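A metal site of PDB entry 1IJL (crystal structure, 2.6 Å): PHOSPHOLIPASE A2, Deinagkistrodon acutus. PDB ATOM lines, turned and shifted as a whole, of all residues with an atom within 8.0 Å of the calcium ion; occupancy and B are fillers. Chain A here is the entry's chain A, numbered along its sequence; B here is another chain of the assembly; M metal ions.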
ATOM      1  N   TYR A  21      15.727   0.550  -9.515  1.00  0.00           N
ATOM      2  CA  TYR A  21      16.907   1.443  -9.672  1.00  0.00           C
ATOM      3  C   TYR A  21      17.119   2.038 -11.084  1.00  0.00           C
ATOM      4  O   TYR A  21      18.181   2.609 -11.380  1.00  0.00           O
ATOM      5  CB  TYR A  21      18.192   0.669  -9.367  1.00  0.00           C
ATOM      6  CG  TYR A  21      18.274   0.205  -7.928  1.00  0.00           C
ATOM      7  CD1 TYR A  21      18.776   1.061  -6.947  1.00  0.00           C
ATOM      8  CD2 TYR A  21      17.838  -1.085  -7.580  1.00  0.00           C
ATOM      9  CE1 TYR A  21      18.845   0.643  -5.625  1.00  0.00           C
ATOM     10  CE2 TYR A  21      17.904  -1.504  -6.249  1.00  0.00           C
ATOM     11  CZ  TYR A  21      18.416  -0.640  -5.273  1.00  0.00           C
ATOM     12  OH  TYR A  21      18.473  -1.047  -3.976  1.00  0.00           O
ATOM     13  N   SER A  22      16.149   1.938 -11.950  1.00  0.00           N
ATOM     14  CA  SER A  22      16.306   2.478 -13.327  1.00  0.00           C
ATOM     15  C   SER A  22      15.718   3.893 -13.443  1.00  0.00           C
ATOM     16  O   SER A  22      15.818   4.541 -14.500  1.00  0.00           O
ATOM     17  CB  SER A  22      15.611   1.593 -14.346  1.00  0.00           C
ATOM     18  OG  SER A  22      14.253   1.396 -13.969  1.00  0.00           O
ATOM     19  N   TYR A  24      15.784   6.281 -10.359  1.00  0.00           N
ATOM     20  CA  TYR A  24      15.903   6.766  -8.999  1.00  0.00           C
ATOM     21  C   TYR A  24      16.872   7.926  -8.841  1.00  0.00           C
ATOM     22  O   TYR A  24      17.993   7.895  -9.368  1.00  0.00           O
ATOM     23  CB  TYR A  24      16.365   5.593  -8.126  1.00  0.00           C
ATOM     24  CG  TYR A  24      16.332   5.831  -6.647  1.00  0.00           C
ATOM     25  CD1 TYR A  24      15.278   5.350  -5.867  1.00  0.00           C
ATOM     26  CD2 TYR A  24      17.387   6.488  -6.009  1.00  0.00           C
ATOM     27  CE1 TYR A  24      15.280   5.522  -4.471  1.00  0.00           C
ATOM     28  CE2 TYR A  24      17.407   6.670  -4.637  1.00  0.00           C
ATOM     29  CZ  TYR A  24      16.350   6.184  -3.870  1.00  0.00           C
ATOM     30  OH  TYR A  24      16.393   6.346  -2.502  1.00  0.00           O
ATOM     31  N   CYS A  26      19.018  11.330  -9.025  1.00  0.00           N
ATOM     32  CA  CYS A  26      19.601  12.057 -10.139  1.00  0.00           C
ATOM     33  C   CYS A  26      20.567  11.266 -11.018  1.00  0.00           C
ATOM     34  O   CYS A  26      20.894  11.700 -12.126  1.00  0.00           O
ATOM     35  CB  CYS A  26      20.315  13.306  -9.623  1.00  0.00           C
ATOM     36  SG  CYS A  26      19.228  14.641  -9.069  1.00  0.00           S
ATOM     37  N   TYR A  27      21.011  10.109 -10.528  1.00  0.00           N
ATOM     38  CA  TYR A  27      21.980   9.305 -11.277  1.00  0.00           C
ATOM     39  C   TYR A  27      21.580   7.869 -11.557  1.00  0.00           C
ATOM     40  O   TYR A  27      22.143   7.235 -12.429  1.00  0.00           O
ATOM     41  CB  TYR A  27      23.337   9.340 -10.560  1.00  0.00           C
ATOM     42  CG  TYR A  27      24.068  10.654 -10.744  1.00  0.00           C
ATOM     43  CD1 TYR A  27      24.887  10.859 -11.865  1.00  0.00           C
ATOM     44  CD2 TYR A  27      23.888  11.712  -9.850  1.00  0.00           C
ATOM     45  CE1 TYR A  27      25.505  12.092 -12.085  1.00  0.00           C
ATOM     46  CE2 TYR A  27      24.499  12.953 -10.071  1.00  0.00           C
ATOM     47  CZ  TYR A  27      25.308  13.122 -11.191  1.00  0.00           C
ATOM     48  OH  TYR A  27      25.906  14.336 -11.421  1.00  0.00           O
ATOM     49  N   CYS A  28      20.627   7.349 -10.808  1.00  0.00           N
ATOM     50  CA  CYS A  28      20.196   5.976 -11.035  1.00  0.00           C
ATOM     51  C   CYS A  28      19.241   5.975 -12.218  1.00  0.00           C
ATOM     52  O   CYS A  28      18.055   6.288 -12.087  1.00  0.00           O
ATOM     53  CB  CYS A  28      19.533   5.408  -9.788  1.00  0.00           C
ATOM     54  SG  CYS A  28      20.645   5.261  -8.348  1.00  0.00           S
ATOM     55  N   GLY A  29      19.783   5.643 -13.379  1.00  0.00           N
ATOM     56  CA  GLY A  29      19.020   5.641 -14.606  1.00  0.00           C
ATOM     57  C   GLY A  29      19.986   6.022 -15.707  1.00  0.00           C
ATOM     58  O   GLY A  29      21.172   6.210 -15.425  1.00  0.00           O
ATOM     59  N   TRP A  30      19.521   6.148 -16.937  1.00  0.00           N
ATOM     60  CA  TRP A  30      20.446   6.482 -18.019  1.00  0.00           C
ATOM     61  C   TRP A  30      20.963   7.914 -17.944  1.00  0.00           C
ATOM     62  O   TRP A  30      20.179   8.862 -17.904  1.00  0.00           O
ATOM     63  CB  TRP A  30      19.795   6.229 -19.380  1.00  0.00           C
ATOM     64  CG  TRP A  30      20.814   5.922 -20.435  1.00  0.00           C
ATOM     65  CD1 TRP A  30      21.384   6.806 -21.313  1.00  0.00           C
ATOM     66  CD2 TRP A  30      21.461   4.671 -20.641  1.00  0.00           C
ATOM     67  NE1 TRP A  30      22.347   6.173 -22.060  1.00  0.00           N
ATOM     68  CE2 TRP A  30      22.423   4.860 -21.664  1.00  0.00           C
ATOM     69  CE3 TRP A  30      21.341   3.396 -20.067  1.00  0.00           C
ATOM     70  CZ2 TRP A  30      23.243   3.820 -22.128  1.00  0.00           C
ATOM     71  CZ3 TRP A  30      22.147   2.374 -20.512  1.00  0.00           C
ATOM     72  CH2 TRP A  30      23.097   2.592 -21.536  1.00  0.00           C
ATOM     73  N   GLY A  31      22.277   8.057 -17.922  1.00  0.00           N
ATOM     74  CA  GLY A  31      22.870   9.380 -17.844  1.00  0.00           C
ATOM     75  C   GLY A  31      22.970   9.824 -16.401  1.00  0.00           C
ATOM     76  O   GLY A  31      23.157   9.006 -15.506  1.00  0.00           O
ATOM     77  N   GLY A  32      22.850  11.127 -16.174  1.00  0.00           N
ATOM     78  CA  GLY A  32      22.964  11.643 -14.834  1.00  0.00           C
ATOM     79  C   GLY A  32      23.504  13.058 -14.882  1.00  0.00           C
ATOM     80  O   GLY A  32      24.332  13.393 -15.731  1.00  0.00           O
ATOM     81  N   HIS A  33      23.074  13.889 -13.949  1.00  0.00           N
ATOM     82  CA  HIS A  33      23.502  15.272 -13.927  1.00  0.00           C
ATOM     83  C   HIS A  33      23.064  15.765 -12.559  1.00  0.00           C
ATOM     84  O   HIS A  33      22.237  15.119 -11.920  1.00  0.00           O
ATOM     85  CB  HIS A  33      22.778  16.014 -15.057  1.00  0.00           C
ATOM     86  CG  HIS A  33      23.360  17.356 -15.382  1.00  0.00           C
ATOM     87  ND1 HIS A  33      23.004  18.499 -14.709  1.00  0.00           N
ATOM     88  CD2 HIS A  33      24.236  17.737 -16.346  1.00  0.00           C
ATOM     89  CE1 HIS A  33      23.641  19.538 -15.243  1.00  0.00           C
ATOM     90  NE2 HIS A  33      24.390  19.100 -16.230  1.00  0.00           N
ATOM     91  N   ASP A  41      21.645   6.877  -4.544  1.00  0.00           N
ATOM     92  CA  ASP A  41      21.943   7.738  -5.685  1.00  0.00           C
ATOM     93  C   ASP A  41      23.457   7.928  -5.838  1.00  0.00           C
ATOM     94  O   ASP A  41      23.961   8.033  -6.948  1.00  0.00           O
ATOM     95  CB  ASP A  41      21.225   9.081  -5.516  1.00  0.00           C
ATOM     96  CG  ASP A  41      20.874   9.750  -6.835  1.00  0.00           C
ATOM     97  OD1 ASP A  41      20.769   9.058  -7.873  1.00  0.00           O
ATOM     98  OD2 ASP A  41      20.661  10.977  -6.852  1.00  0.00           O
ATOM     99  N   CYS A  44      25.081   5.067  -7.694  1.00  0.00           N
ATOM    100  CA  CYS A  44      24.943   5.197  -9.141  1.00  0.00           C
ATOM    101  C   CYS A  44      25.918   6.232  -9.706  1.00  0.00           C
ATOM    102  O   CYS A  44      26.482   6.044 -10.782  1.00  0.00           O
ATOM    103  CB  CYS A  44      23.495   5.581  -9.516  1.00  0.00           C
ATOM    104  SG  CYS A  44      22.295   4.299  -9.057  1.00  0.00           S
ATOM    105  N   PHE A  45      26.126   7.319  -8.968  1.00  0.00           N
ATOM    106  CA  PHE A  45      27.037   8.363  -9.405  1.00  0.00           C
ATOM    107  C   PHE A  45      28.442   7.766  -9.503  1.00  0.00           C
ATOM    108  O   PHE A  45      29.166   7.984 -10.476  1.00  0.00           O
ATOM    109  CB  PHE A  45      26.997   9.527  -8.407  1.00  0.00           C
ATOM    110  CG  PHE A  45      28.076  10.553  -8.594  1.00  0.00           C
ATOM    111  CD1 PHE A  45      29.266  10.481  -7.873  1.00  0.00           C
ATOM    112  CD2 PHE A  45      27.921  11.583  -9.520  1.00  0.00           C
ATOM    113  CE1 PHE A  45      30.274  11.431  -8.067  1.00  0.00           C
ATOM    114  CE2 PHE A  45      28.936  12.539  -9.711  1.00  0.00           C
ATOM    115  CZ  PHE A  45      30.116  12.459  -8.984  1.00  0.00           C
ATOM    116  N   HIS A  47      29.166   4.612  -9.903  1.00  0.00           N
ATOM    117  CA  HIS A  47      29.135   3.617 -10.968  1.00  0.00           C
ATOM    118  C   HIS A  47      29.336   4.282 -12.319  1.00  0.00           C
ATOM    119  O   HIS A  47      30.036   3.746 -13.177  1.00  0.00           O
ATOM    120  CB  HIS A  47      27.811   2.853 -10.947  1.00  0.00           C
ATOM    121  CG  HIS A  47      27.771   1.687 -11.878  1.00  0.00           C
ATOM    122  ND1 HIS A  47      27.365   1.796 -13.186  1.00  0.00           N
ATOM    123  CD2 HIS A  47      28.111   0.391 -11.691  1.00  0.00           C
ATOM    124  CE1 HIS A  47      27.464   0.605 -13.773  1.00  0.00           C
ATOM    125  NE2 HIS A  47      27.901  -0.262 -12.884  1.00  0.00           N
ATOM    126  N   ASP A  48      28.701   5.437 -12.514  1.00  0.00           N
ATOM    127  CA  ASP A  48      28.838   6.205 -13.745  1.00  0.00           C
ATOM    128  C   ASP A  48      30.300   6.654 -13.858  1.00  0.00           C
ATOM    129  O   ASP A  48      30.892   6.611 -14.944  1.00  0.00           O
ATOM    130  CB  ASP A  48      27.937   7.440 -13.708  1.00  0.00           C
ATOM    131  CG  ASP A  48      26.512   7.156 -14.153  1.00  0.00           C
ATOM    132  OD1 ASP A  48      26.015   6.029 -13.935  1.00  0.00           O
ATOM    133  OD2 ASP A  48      25.882   8.062 -14.732  1.00  0.00           O
ATOM    134  N   CYS A  49      30.864   7.080 -12.733  1.00  0.00           N
ATOM    135  CA  CYS A  49      32.250   7.537 -12.668  1.00  0.00           C
ATOM    136  C   CYS A  49      33.206   6.387 -12.931  1.00  0.00           C
ATOM    137  O   CYS A  49      34.292   6.580 -13.470  1.00  0.00           O
ATOM    138  CB  CYS A  49      32.566   8.119 -11.291  1.00  0.00           C
ATOM    139  SG  CYS A  49      31.926   9.790 -10.975  1.00  0.00           S
ATOM    140  N   TRP B  20      14.261  -0.731 -21.362  1.00  0.00           N
ATOM    141  CA  TRP B  20      13.644  -0.745 -20.045  1.00  0.00           C
ATOM    142  C   TRP B  20      12.134  -0.515 -20.109  1.00  0.00           C
ATOM    143  O   TRP B  20      11.642   0.199 -20.977  1.00  0.00           O
ATOM    144  CB  TRP B  20      14.304   0.302 -19.146  1.00  0.00           C
ATOM    145  CG  TRP B  20      15.802   0.210 -19.087  1.00  0.00           C
ATOM    146  CD1 TRP B  20      16.582  -0.825 -19.544  1.00  0.00           C
ATOM    147  CD2 TRP B  20      16.706   1.174 -18.539  1.00  0.00           C
ATOM    148  NE1 TRP B  20      17.901  -0.557 -19.317  1.00  0.00           N
ATOM    149  CE2 TRP B  20      18.021   0.658 -18.704  1.00  0.00           C
ATOM    150  CE3 TRP B  20      16.546   2.425 -17.923  1.00  0.00           C
ATOM    151  CZ2 TRP B  20      19.154   1.354 -18.279  1.00  0.00           C
ATOM    152  CZ3 TRP B  20      17.672   3.115 -17.502  1.00  0.00           C
ATOM    153  CH2 TRP B  20      18.965   2.574 -17.691  1.00  0.00           C
HETATM  154 CA    CA M   1      23.289   7.116 -14.525  1.00  0.00          CA
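The side-chain carboxylate (OD1) of Asp 41 is in hydrogen-bond range of the backbone NH (N) of Tyr 27 (2.9 Å).
The side-chain sulfur of Cys 44 forms a disulfide with the side-chain sulfur of Cys 28 (2.0 Å).
Four residues have an atom within 4 Å of the calcium ion: Tyr 27, Gly 29, Gly 31 and Asp 48.
The calcium ion is bound by the backbone carbonyl oxygen (O) of Gly 31 (2.1 Å).
O of Tyr 27 is bound to the calcium ion (2.4 Å).
O of Gly 29 binds the calcium ion (2.5 Å).
The calcium ion is bound by OD2 of Asp 48, 2.8 Å away.
Slightly farther from the calcium ion lies OD1 of Asp 48 (3.0 Å).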
